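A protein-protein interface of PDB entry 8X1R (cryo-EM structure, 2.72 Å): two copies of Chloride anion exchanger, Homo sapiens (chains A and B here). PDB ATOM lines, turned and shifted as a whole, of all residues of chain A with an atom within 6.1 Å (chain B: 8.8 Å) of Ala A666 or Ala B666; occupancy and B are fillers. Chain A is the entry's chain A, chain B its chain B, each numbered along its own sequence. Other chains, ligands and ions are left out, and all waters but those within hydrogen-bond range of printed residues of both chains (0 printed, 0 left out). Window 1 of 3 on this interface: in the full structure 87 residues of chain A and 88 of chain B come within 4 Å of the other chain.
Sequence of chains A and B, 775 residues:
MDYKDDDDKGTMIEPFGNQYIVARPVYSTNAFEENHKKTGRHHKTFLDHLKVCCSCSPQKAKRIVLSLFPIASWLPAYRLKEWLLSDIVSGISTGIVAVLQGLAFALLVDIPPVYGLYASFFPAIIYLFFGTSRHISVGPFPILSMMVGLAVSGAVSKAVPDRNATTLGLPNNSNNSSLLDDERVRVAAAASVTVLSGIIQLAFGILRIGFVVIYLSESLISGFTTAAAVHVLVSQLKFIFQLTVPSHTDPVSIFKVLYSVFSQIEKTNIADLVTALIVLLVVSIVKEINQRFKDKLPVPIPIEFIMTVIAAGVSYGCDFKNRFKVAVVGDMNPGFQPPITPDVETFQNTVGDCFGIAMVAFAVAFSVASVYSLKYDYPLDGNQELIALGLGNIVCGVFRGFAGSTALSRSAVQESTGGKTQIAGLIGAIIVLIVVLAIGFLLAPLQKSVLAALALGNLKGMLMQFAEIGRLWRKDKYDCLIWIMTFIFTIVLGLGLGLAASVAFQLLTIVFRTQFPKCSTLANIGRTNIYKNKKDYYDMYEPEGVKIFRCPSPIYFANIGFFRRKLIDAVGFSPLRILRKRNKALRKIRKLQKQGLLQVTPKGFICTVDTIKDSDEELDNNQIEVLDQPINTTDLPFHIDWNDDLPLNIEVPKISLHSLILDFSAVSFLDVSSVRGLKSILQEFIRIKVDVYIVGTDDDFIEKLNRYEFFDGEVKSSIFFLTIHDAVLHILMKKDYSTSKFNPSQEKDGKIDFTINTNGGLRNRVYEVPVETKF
Of the 22 printed residues of chain B, 7 touch a printed residue of chain A.
Printed residues of chain A that touch a printed residue of chain B: Arg A550, Pro A552, Ser A553, Pro A554, Ser A665, Ala A666 and Ser A668.
Hydrophobic or aromatic side chains of chain A within 4 Å of the printed part of chain B: Pro A554 and Ala A666.
Among the printed residues, 15 pairs touch across the chains.
Among the printed residues, Asp or Glu carboxylates within 4 Å of a Lys or Arg side-chain nitrogen of the other chain: Arg A550 with Asp B698 (3.8 Å).
The side-chain carboxylate (OD2) of Asp B698 is in salt-bridge range of the guanidinium group (NH1) of Arg A550 (3.8 Å).
The backbone carbonyl oxygen of Ala A666 is in hydrogen-bond range of the side-chain hydroxyl of Ser B668, 3.1 Å away.
The backbone carbonyl oxygen of Ala B666 lies within hydrogen-bond range of the side-chain hydroxyl of Ser A668.
Ala A666 touches three residues of chain B.
Ala B666 touches three residues of chain A.
Printed residues of chain A within 4 Å of Ser B668: Pro A552 (3.5 Å), Ser A553 (3.6 Å), Pro A554 (3.3 Å), Ala A666 (3.1 Å) and Ser A668 (3.7 Å).
Printed residues of chain A within 4 Å of Asp B698: Arg A550.
The nearest printed residue of chain B that does not touch Pro A552 is Asp B698 (4.5 Å).
The guanidinium group of Arg A550 is in salt-bridge range of the side-chain carboxylate of Asp A663, 2.7 Å away.
NH2 of Arg A550 is in hydrogen-bond range of OG of Ser A665 (3.1 Å).
ND2 of Asn B559 is in hydrogen-bond range of OG of Ser B553 (3.4 Å).
The backbone carbonyl oxygen (O) of Pro B554 is in hydrogen-bond range of the side-chain amide nitrogen (ND2) of Asn B559.
OD1 of Asp B663 is in hydrogen-bond range of OG of Ser B665 (2.7 Å).
Ser A553 touches Ser B668, and with the chains exchanged Ser A668 touches Ser B553.
Pro A554 touches Ser B668, and with the chains exchanged Ser A668 touches Pro B554.
Ser B665 touches its own counterpart, Ser A665.
Ala A666 touches Ser B668, and with the chains exchanged Ser A668 touches Ala B666.
Of the 15 pairs that touch across the chains among the printed residues, 14 have their exchanged pair printed and touching as well.
Pro A552 touches Ser B668.
Pro A554 touches Pro B554 (CG to CG, 3.8 Å).
OG of Ser B668 touches CD of Pro A554, at 3.3 Å.
Ser B665 touches Ser A665.
O of Ser A665 touches CB of Ala B666 (3.6 Å).
CA of Ala A666 touches CA of Ala B666, at 3.8 Å.
Ser A668 touches Pro B552.
CA of Ser B553 touches OG of Ser A668, 3.3 Å away.
Ser A668 touches Pro B554 (OG to CD, 3.1 Å).
OG of Ser B668 touches OG of Ser A668, 3.7 Å away.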
ATOM      1  N   ARG A 550      20.493 -14.499 -24.251  1.00  0.00           N
ATOM      2  CA  ARG A 550      19.652 -15.625 -24.624  1.00  0.00           C
ATOM      3  C   ARG A 550      20.487 -16.677 -25.338  1.00  0.00           C
ATOM      4  O   ARG A 550      21.155 -16.376 -26.332  1.00  0.00           O
ATOM      5  CB  ARG A 550      18.496 -15.170 -25.512  1.00  0.00           C
ATOM      6  CG  ARG A 550      17.925 -16.268 -26.371  1.00  0.00           C
ATOM      7  CD  ARG A 550      16.689 -15.814 -27.110  1.00  0.00           C
ATOM      8  NE  ARG A 550      16.027 -16.926 -27.778  1.00  0.00           N
ATOM      9  CZ  ARG A 550      15.042 -17.633 -27.241  1.00  0.00           C
ATOM     10  NH1 ARG A 550      14.497 -18.633 -27.912  1.00  0.00           N
ATOM     11  NH2 ARG A 550      14.604 -17.339 -26.028  1.00  0.00           N
ATOM     12  N   CYS A 551      20.456 -17.903 -24.819  1.00  0.00           N
ATOM     13  CA  CYS A 551      20.967 -19.078 -25.508  1.00  0.00           C
ATOM     14  C   CYS A 551      19.784 -19.913 -25.966  1.00  0.00           C
ATOM     15  O   CYS A 551      19.006 -20.382 -25.122  1.00  0.00           O
ATOM     16  CB  CYS A 551      21.879 -19.899 -24.602  1.00  0.00           C
ATOM     17  SG  CYS A 551      22.576 -21.369 -25.384  1.00  0.00           S
ATOM     18  N   PRO A 552      19.581 -20.102 -27.268  1.00  0.00           N
ATOM     19  CA  PRO A 552      18.374 -20.764 -27.772  1.00  0.00           C
ATOM     20  C   PRO A 552      18.509 -22.277 -27.924  1.00  0.00           C
ATOM     21  O   PRO A 552      18.129 -22.852 -28.948  1.00  0.00           O
ATOM     22  CB  PRO A 552      18.174 -20.090 -29.129  1.00  0.00           C
ATOM     23  CG  PRO A 552      19.577 -19.862 -29.596  1.00  0.00           C
ATOM     24  CD  PRO A 552      20.432 -19.629 -28.372  1.00  0.00           C
ATOM     25  N   SER A 553      19.086 -22.953 -26.939  1.00  0.00           N
ATOM     26  CA  SER A 553      19.224 -24.412 -26.994  1.00  0.00           C
ATOM     27  C   SER A 553      19.473 -24.955 -25.616  1.00  0.00           C
ATOM     28  O   SER A 553      19.811 -24.197 -24.728  1.00  0.00           O
ATOM     29  CB  SER A 553      20.373 -24.873 -27.913  1.00  0.00           C
ATOM     30  OG  SER A 553      21.628 -24.615 -27.347  1.00  0.00           O
ATOM     31  N   PRO A 554      19.276 -26.273 -25.431  1.00  0.00           N
ATOM     32  CA  PRO A 554      19.559 -26.936 -24.159  1.00  0.00           C
ATOM     33  C   PRO A 554      21.016 -26.653 -23.991  1.00  0.00           C
ATOM     34  O   PRO A 554      21.776 -27.068 -24.846  1.00  0.00           O
ATOM     35  CB  PRO A 554      19.390 -28.407 -24.486  1.00  0.00           C
ATOM     36  CG  PRO A 554      18.538 -28.456 -25.690  1.00  0.00           C
ATOM     37  CD  PRO A 554      18.801 -27.211 -26.459  1.00  0.00           C
ATOM     38  N   ASP A 663      17.956 -15.329 -20.346  1.00  0.00           N
ATOM     39  CA  ASP A 663      16.697 -15.820 -20.901  1.00  0.00           C
ATOM     40  C   ASP A 663      16.827 -17.317 -21.141  1.00  0.00           C
ATOM     41  O   ASP A 663      17.224 -17.756 -22.221  1.00  0.00           O
ATOM     42  CB  ASP A 663      16.354 -15.072 -22.183  1.00  0.00           C
ATOM     43  CG  ASP A 663      15.069 -15.553 -22.812  1.00  0.00           C
ATOM     44  OD1 ASP A 663      14.171 -15.996 -22.068  1.00  0.00           O
ATOM     45  OD2 ASP A 663      14.950 -15.482 -24.052  1.00  0.00           O
ATOM     46  N   PHE A 664      16.479 -18.111 -20.129  1.00  0.00           N
ATOM     47  CA  PHE A 664      16.593 -19.563 -20.176  1.00  0.00           C
ATOM     48  C   PHE A 664      15.314 -20.222 -20.672  1.00  0.00           C
ATOM     49  O   PHE A 664      15.021 -21.363 -20.304  1.00  0.00           O
ATOM     50  CB  PHE A 664      16.963 -20.106 -18.797  1.00  0.00           C
ATOM     51  CG  PHE A 664      18.433 -20.319 -18.595  1.00  0.00           C
ATOM     52  CD1 PHE A 664      19.360 -19.474 -19.170  1.00  0.00           C
ATOM     53  CD2 PHE A 664      18.886 -21.367 -17.821  1.00  0.00           C
ATOM     54  CE1 PHE A 664      20.705 -19.674 -18.978  1.00  0.00           C
ATOM     55  CE2 PHE A 664      20.229 -21.568 -17.629  1.00  0.00           C
ATOM     56  CZ  PHE A 664      21.138 -20.721 -18.207  1.00  0.00           C
ATOM     57  N   SER A 665      14.545 -19.521 -21.505  1.00  0.00           N
ATOM     58  CA  SER A 665      13.246 -20.029 -21.930  1.00  0.00           C
ATOM     59  C   SER A 665      13.385 -21.213 -22.875  1.00  0.00           C
ATOM     60  O   SER A 665      12.695 -22.225 -22.712  1.00  0.00           O
ATOM     61  CB  SER A 665      12.443 -18.914 -22.587  1.00  0.00           C
ATOM     62  OG  SER A 665      12.797 -18.776 -23.948  1.00  0.00           O
ATOM     63  N   ALA A 666      14.264 -21.110 -23.867  1.00  0.00           N
ATOM     64  CA  ALA A 666      14.470 -22.181 -24.829  1.00  0.00           C
ATOM     65  C   ALA A 666      15.528 -23.177 -24.390  1.00  0.00           C
ATOM     66  O   ALA A 666      15.850 -24.089 -25.153  1.00  0.00           O
ATOM     67  CB  ALA A 666      14.850 -21.609 -26.194  1.00  0.00           C
ATOM     68  N   VAL A 667      16.080 -23.025 -23.188  1.00  0.00           N
ATOM     69  CA  VAL A 667      17.047 -23.978 -22.652  1.00  0.00           C
ATOM     70  C   VAL A 667      16.252 -25.149 -22.087  1.00  0.00           C
ATOM     71  O   VAL A 667      15.615 -25.038 -21.041  1.00  0.00           O
ATOM     72  CB  VAL A 667      17.956 -23.345 -21.599  1.00  0.00           C
ATOM     73  CG1 VAL A 667      18.795 -24.403 -20.938  1.00  0.00           C
ATOM     74  CG2 VAL A 667      18.840 -22.297 -22.237  1.00  0.00           C
ATOM     75  N   SER A 668      16.287 -26.280 -22.789  1.00  0.00           N
ATOM     76  CA  SER A 668      15.451 -27.420 -22.439  1.00  0.00           C
ATOM     77  C   SER A 668      15.955 -28.122 -21.183  1.00  0.00           C
ATOM     78  O   SER A 668      15.240 -28.208 -20.180  1.00  0.00           O
ATOM     79  CB  SER A 668      15.393 -28.393 -23.614  1.00  0.00           C
ATOM     80  OG  SER A 668      14.699 -27.812 -24.700  1.00  0.00           O
ATOM     81  N   GLY A 696      12.080 -17.053 -17.693  1.00  0.00           N
ATOM     82  CA  GLY A 696      11.487 -17.839 -18.753  1.00  0.00           C
ATOM     83  C   GLY A 696      11.470 -19.338 -18.595  1.00  0.00           C
ATOM     84  O   GLY A 696      11.076 -20.048 -19.506  1.00  0.00           O
ATOM     85  N   THR B 514      15.750 -36.236 -24.283  1.00  0.00           N
ATOM     86  CA  THR B 514      14.688 -35.630 -25.070  1.00  0.00           C
ATOM     87  C   THR B 514      13.852 -36.660 -25.816  1.00  0.00           C
ATOM     88  O   THR B 514      13.424 -36.397 -26.942  1.00  0.00           O
ATOM     89  CB  THR B 514      15.285 -34.623 -26.053  1.00  0.00           C
ATOM     90  OG1 THR B 514      16.475 -35.166 -26.627  1.00  0.00           O
ATOM     91  CG2 THR B 514      15.631 -33.335 -25.343  1.00  0.00           C
ATOM     92  N   PRO B 517       9.390 -36.417 -23.739  1.00  0.00           N
ATOM     93  CA  PRO B 517       9.317 -35.142 -23.018  1.00  0.00           C
ATOM     94  C   PRO B 517       8.038 -35.039 -22.206  1.00  0.00           C
ATOM     95  O   PRO B 517       6.994 -35.573 -22.584  1.00  0.00           O
ATOM     96  CB  PRO B 517       9.357 -34.094 -24.134  1.00  0.00           C
ATOM     97  CG  PRO B 517       9.670 -34.827 -25.376  1.00  0.00           C
ATOM     98  CD  PRO B 517       9.248 -36.232 -25.189  1.00  0.00           C
ATOM     99  N   ARG B 550       2.217 -27.597 -24.409  1.00  0.00           N
ATOM    100  CA  ARG B 550       3.629 -27.259 -24.313  1.00  0.00           C
ATOM    101  C   ARG B 550       4.464 -28.527 -24.376  1.00  0.00           C
ATOM    102  O   ARG B 550       4.268 -29.443 -23.575  1.00  0.00           O
ATOM    103  CB  ARG B 550       3.909 -26.497 -23.020  1.00  0.00           C
ATOM    104  CG  ARG B 550       5.371 -26.255 -22.767  1.00  0.00           C
ATOM    105  CD  ARG B 550       5.603 -25.606 -21.427  1.00  0.00           C
ATOM    106  NE  ARG B 550       6.997 -25.717 -21.024  1.00  0.00           N
ATOM    107  CZ  ARG B 550       7.943 -24.852 -21.367  1.00  0.00           C
ATOM    108  NH1 ARG B 550       9.186 -25.032 -20.954  1.00  0.00           N
ATOM    109  NH2 ARG B 550       7.646 -23.805 -22.119  1.00  0.00           N
ATOM    110  N   CYS B 551       5.376 -28.587 -25.344  1.00  0.00           N
ATOM    111  CA  CYS B 551       6.427 -29.594 -25.372  1.00  0.00           C
ATOM    112  C   CYS B 551       7.735 -28.926 -24.984  1.00  0.00           C
ATOM    113  O   CYS B 551       8.197 -28.028 -25.703  1.00  0.00           O
ATOM    114  CB  CYS B 551       6.544 -30.237 -26.751  1.00  0.00           C
ATOM    115  SG  CYS B 551       7.798 -31.533 -26.866  1.00  0.00           S
ATOM    116  N   PRO B 552       8.281 -29.288 -23.818  1.00  0.00           N
ATOM    117  CA  PRO B 552       9.464 -28.681 -23.213  1.00  0.00           C
ATOM    118  C   PRO B 552      10.829 -29.074 -23.732  1.00  0.00           C
ATOM    119  O   PRO B 552      11.743 -29.151 -22.925  1.00  0.00           O
ATOM    120  CB  PRO B 552       9.340 -29.102 -21.758  1.00  0.00           C
ATOM    121  CG  PRO B 552       8.665 -30.416 -21.820  1.00  0.00           C
ATOM    122  CD  PRO B 552       7.740 -30.374 -22.991  1.00  0.00           C
ATOM    123  N   SER B 553      10.955 -29.388 -25.016  1.00  0.00           N
ATOM    124  CA  SER B 553      12.233 -29.806 -25.572  1.00  0.00           C
ATOM    125  C   SER B 553      12.266 -29.680 -27.074  1.00  0.00           C
ATOM    126  O   SER B 553      11.230 -29.574 -27.694  1.00  0.00           O
ATOM    127  CB  SER B 553      12.516 -31.265 -25.217  1.00  0.00           C
ATOM    128  OG  SER B 553      11.863 -32.136 -26.110  1.00  0.00           O
ATOM    129  N   PRO B 554      13.474 -29.698 -27.664  1.00  0.00           N
ATOM    130  CA  PRO B 554      13.630 -29.627 -29.113  1.00  0.00           C
ATOM    131  C   PRO B 554      12.938 -30.831 -29.661  1.00  0.00           C
ATOM    132  O   PRO B 554      13.207 -31.919 -29.184  1.00  0.00           O
ATOM    133  CB  PRO B 554      15.118 -29.844 -29.319  1.00  0.00           C
ATOM    134  CG  PRO B 554      15.751 -29.529 -28.031  1.00  0.00           C
ATOM    135  CD  PRO B 554      14.759 -29.863 -26.975  1.00  0.00           C
ATOM    136  N   ILE B 555      12.075 -30.686 -30.642  1.00  0.00           N
ATOM    137  CA  ILE B 555      11.420 -31.866 -31.142  1.00  0.00           C
ATOM    138  C   ILE B 555      12.245 -32.368 -32.296  1.00  0.00           C
ATOM    139  O   ILE B 555      12.390 -31.656 -33.268  1.00  0.00           O
ATOM    140  CB  ILE B 555      10.013 -31.526 -31.667  1.00  0.00           C
ATOM    141  CG1 ILE B 555       9.201 -30.787 -30.612  1.00  0.00           C
ATOM    142  CG2 ILE B 555       9.266 -32.774 -32.087  1.00  0.00           C
ATOM    143  CD1 ILE B 555       7.887 -30.266 -31.130  1.00  0.00           C
ATOM    144  N   ASN B 559      11.330 -37.729 -31.391  1.00  0.00           N
ATOM    145  CA  ASN B 559      10.442 -36.957 -30.538  1.00  0.00           C
ATOM    146  C   ASN B 559       9.050 -36.762 -31.098  1.00  0.00           C
ATOM    147  O   ASN B 559       8.143 -36.438 -30.325  1.00  0.00           O
ATOM    148  CB  ASN B 559      11.044 -35.569 -30.289  1.00  0.00           C
ATOM    149  CG  ASN B 559      11.372 -35.337 -28.863  1.00  0.00           C
ATOM    150  OD1 ASN B 559      10.853 -36.014 -27.989  1.00  0.00           O
ATOM    151  ND2 ASN B 559      12.244 -34.379 -28.605  1.00  0.00           N
ATOM    152  N   LEU B 662       0.094 -23.866 -29.410  1.00  0.00           N
ATOM    153  CA  LEU B 662       1.274 -24.691 -29.189  1.00  0.00           C
ATOM    154  C   LEU B 662       2.382 -23.795 -28.657  1.00  0.00           C
ATOM    155  O   LEU B 662       2.867 -22.912 -29.367  1.00  0.00           O
ATOM    156  CB  LEU B 662       1.701 -25.390 -30.476  1.00  0.00           C
ATOM    157  CG  LEU B 662       0.744 -26.410 -31.088  1.00  0.00           C
ATOM    158  CD1 LEU B 662       1.188 -26.732 -32.490  1.00  0.00           C
ATOM    159  CD2 LEU B 662       0.696 -27.663 -30.253  1.00  0.00           C
ATOM    160  N   ASP B 663       2.781 -24.019 -27.410  1.00  0.00           N
ATOM    161  CA  ASP B 663       3.802 -23.197 -26.767  1.00  0.00           C
ATOM    162  C   ASP B 663       5.171 -23.744 -27.142  1.00  0.00           C
ATOM    163  O   ASP B 663       5.705 -24.634 -26.479  1.00  0.00           O
ATOM    164  CB  ASP B 663       3.604 -23.176 -25.259  1.00  0.00           C
ATOM    165  CG  ASP B 663       4.675 -22.386 -24.545  1.00  0.00           C
ATOM    166  OD1 ASP B 663       5.097 -21.342 -25.079  1.00  0.00           O
ATOM    167  OD2 ASP B 663       5.090 -22.801 -23.445  1.00  0.00           O
ATOM    168  N   PHE B 664       5.752 -23.195 -28.208  1.00  0.00           N
ATOM    169  CA  PHE B 664       7.027 -23.649 -28.744  1.00  0.00           C
ATOM    170  C   PHE B 664       8.204 -22.882 -28.155  1.00  0.00           C
ATOM    171  O   PHE B 664       9.236 -22.732 -28.814  1.00  0.00           O
ATOM    172  CB  PHE B 664       7.020 -23.529 -30.267  1.00  0.00           C
ATOM    173  CG  PHE B 664       6.574 -24.773 -30.978  1.00  0.00           C
ATOM    174  CD1 PHE B 664       5.687 -25.649 -30.386  1.00  0.00           C
ATOM    175  CD2 PHE B 664       7.041 -25.062 -32.245  1.00  0.00           C
ATOM    176  CE1 PHE B 664       5.282 -26.788 -31.038  1.00  0.00           C
ATOM    177  CE2 PHE B 664       6.637 -26.200 -32.898  1.00  0.00           C
ATOM    178  CZ  PHE B 664       5.756 -27.062 -32.293  1.00  0.00           C
ATOM    179  N   SER B 665       8.062 -22.391 -26.922  1.00  0.00           N
ATOM    180  CA  SER B 665       9.119 -21.605 -26.291  1.00  0.00           C
ATOM    181  C   SER B 665      10.398 -22.411 -26.132  1.00  0.00           C
ATOM    182  O   SER B 665      11.483 -21.938 -26.488  1.00  0.00           O
ATOM    183  CB  SER B 665       8.653 -21.094 -24.929  1.00  0.00           C
ATOM    184  OG  SER B 665       7.538 -20.234 -25.056  1.00  0.00           O
ATOM    185  N   ALA B 666      10.296 -23.624 -25.598  1.00  0.00           N
ATOM    186  CA  ALA B 666      11.459 -24.452 -25.325  1.00  0.00           C
ATOM    187  C   ALA B 666      11.781 -25.421 -26.449  1.00  0.00           C
ATOM    188  O   ALA B 666      12.663 -26.264 -26.278  1.00  0.00           O
ATOM    189  CB  ALA B 666      11.261 -25.229 -24.024  1.00  0.00           C
ATOM    190  N   VAL B 667      11.091 -25.333 -27.583  1.00  0.00           N
ATOM    191  CA  VAL B 667      11.421 -26.141 -28.755  1.00  0.00           C
ATOM    192  C   VAL B 667      12.574 -25.436 -29.461  1.00  0.00           C
ATOM    193  O   VAL B 667      12.374 -24.466 -30.192  1.00  0.00           O
ATOM    194  CB  VAL B 667      10.217 -26.334 -29.680  1.00  0.00           C
ATOM    195  CG1 VAL B 667      10.631 -27.043 -30.950  1.00  0.00           C
ATOM    196  CG2 VAL B 667       9.135 -27.119 -28.974  1.00  0.00           C
ATOM    197  N   SER B 668      13.793 -25.922 -29.233  1.00  0.00           N
ATOM    198  CA  SER B 668      14.983 -25.247 -29.736  1.00  0.00           C
ATOM    199  C   SER B 668      15.117 -25.400 -31.246  1.00  0.00           C
ATOM    200  O   SER B 668      15.357 -24.423 -31.960  1.00  0.00           O
ATOM    201  CB  SER B 668      16.224 -25.788 -29.028  1.00  0.00           C
ATOM    202  OG  SER B 668      16.004 -25.879 -27.634  1.00  0.00           O
ATOM    203  N   PHE B 669      14.976 -26.620 -31.751  1.00  0.00           N
ATOM    204  CA  PHE B 669      15.130 -26.880 -33.171  1.00  0.00           C
ATOM    205  C   PHE B 669      14.109 -27.910 -33.630  1.00  0.00           C
ATOM    206  O   PHE B 669      13.464 -28.588 -32.829  1.00  0.00           O
ATOM    207  CB  PHE B 669      16.556 -27.345 -33.513  1.00  0.00           C
ATOM    208  CG  PHE B 669      16.970 -28.629 -32.842  1.00  0.00           C
ATOM    209  CD1 PHE B 669      16.621 -29.856 -33.377  1.00  0.00           C
ATOM    210  CD2 PHE B 669      17.741 -28.606 -31.698  1.00  0.00           C
ATOM    211  CE1 PHE B 669      17.008 -31.027 -32.774  1.00  0.00           C
ATOM    212  CE2 PHE B 669      18.133 -29.776 -31.094  1.00  0.00           C
ATOM    213  CZ  PHE B 669      17.766 -30.988 -31.635  1.00  0.00           C
ATOM    214  N   VAL B 695       3.220 -20.192 -30.613  1.00  0.00           N
ATOM    215  CA  VAL B 695       3.615 -19.016 -29.857  1.00  0.00           C
ATOM    216  C   VAL B 695       4.951 -19.279 -29.176  1.00  0.00           C
ATOM    217  O   VAL B 695       5.379 -20.421 -29.008  1.00  0.00           O
ATOM    218  CB  VAL B 695       2.546 -18.626 -28.820  1.00  0.00           C
ATOM    219  CG1 VAL B 695       1.211 -18.407 -29.493  1.00  0.00           C
ATOM    220  CG2 VAL B 695       2.426 -19.701 -27.778  1.00  0.00           C
ATOM    221  N   GLY B 696       5.613 -18.194 -28.787  1.00  0.00           N
ATOM    222  CA  GLY B 696       6.836 -18.284 -28.018  1.00  0.00           C
ATOM    223  C   GLY B 696       8.102 -18.467 -28.818  1.00  0.00           C
ATOM    224  O   GLY B 696       9.174 -18.609 -28.221  1.00  0.00           O
ATOM    225  N   THR B 697       8.024 -18.457 -30.142  1.00  0.00           N
ATOM    226  CA  THR B 697       9.179 -18.693 -30.992  1.00  0.00           C
ATOM    227  C   THR B 697       9.869 -17.383 -31.347  1.00  0.00           C
ATOM    228  O   THR B 697       9.229 -16.338 -31.485  1.00  0.00           O
ATOM    229  CB  THR B 697       8.760 -19.409 -32.274  1.00  0.00           C
ATOM    230  OG1 THR B 697       7.617 -18.754 -32.833  1.00  0.00           O
ATOM    231  CG2 THR B 697       8.405 -20.835 -31.977  1.00  0.00           C
ATOM    232  N   ASP B 698      11.190 -17.451 -31.495  1.00  0.00           N
ATOM    233  CA  ASP B 698      11.965 -16.302 -31.929  1.00  0.00           C
ATOM    234  C   ASP B 698      11.922 -16.193 -33.451  1.00  0.00           C
ATOM    235  O   ASP B 698      11.327 -17.022 -34.143  1.00  0.00           O
ATOM    236  CB  ASP B 698      13.398 -16.399 -31.415  1.00  0.00           C
ATOM    237  CG  ASP B 698      13.955 -17.799 -31.508  1.00  0.00           C
ATOM    238  OD1 ASP B 698      15.186 -17.942 -31.672  1.00  0.00           O
ATOM    239  OD2 ASP B 698      13.162 -18.758 -31.421  1.00  0.00           O
ATOM    240  N   PHE B 701      13.628 -19.026 -35.552  1.00  0.00           N
ATOM    241  CA  PHE B 701      12.823 -20.234 -35.693  1.00  0.00           C
ATOM    242  C   PHE B 701      11.930 -20.159 -36.926  1.00  0.00           C
ATOM    243  O   PHE B 701      11.868 -21.100 -37.722  1.00  0.00           O
ATOM    244  CB  PHE B 701      11.990 -20.436 -34.427  1.00  0.00           C
ATOM    245  CG  PHE B 701      11.362 -21.793 -34.314  1.00  0.00           C
ATOM    246  CD1 PHE B 701      10.090 -22.024 -34.806  1.00  0.00           C
ATOM    247  CD2 PHE B 701      12.033 -22.833 -33.699  1.00  0.00           C
ATOM    248  CE1 PHE B 701       9.511 -23.259 -34.696  1.00  0.00           C
ATOM    249  CE2 PHE B 701      11.453 -24.072 -33.589  1.00  0.00           C
ATOM    250  CZ  PHE B 701      10.193 -24.284 -34.087  1.00  0.00           C
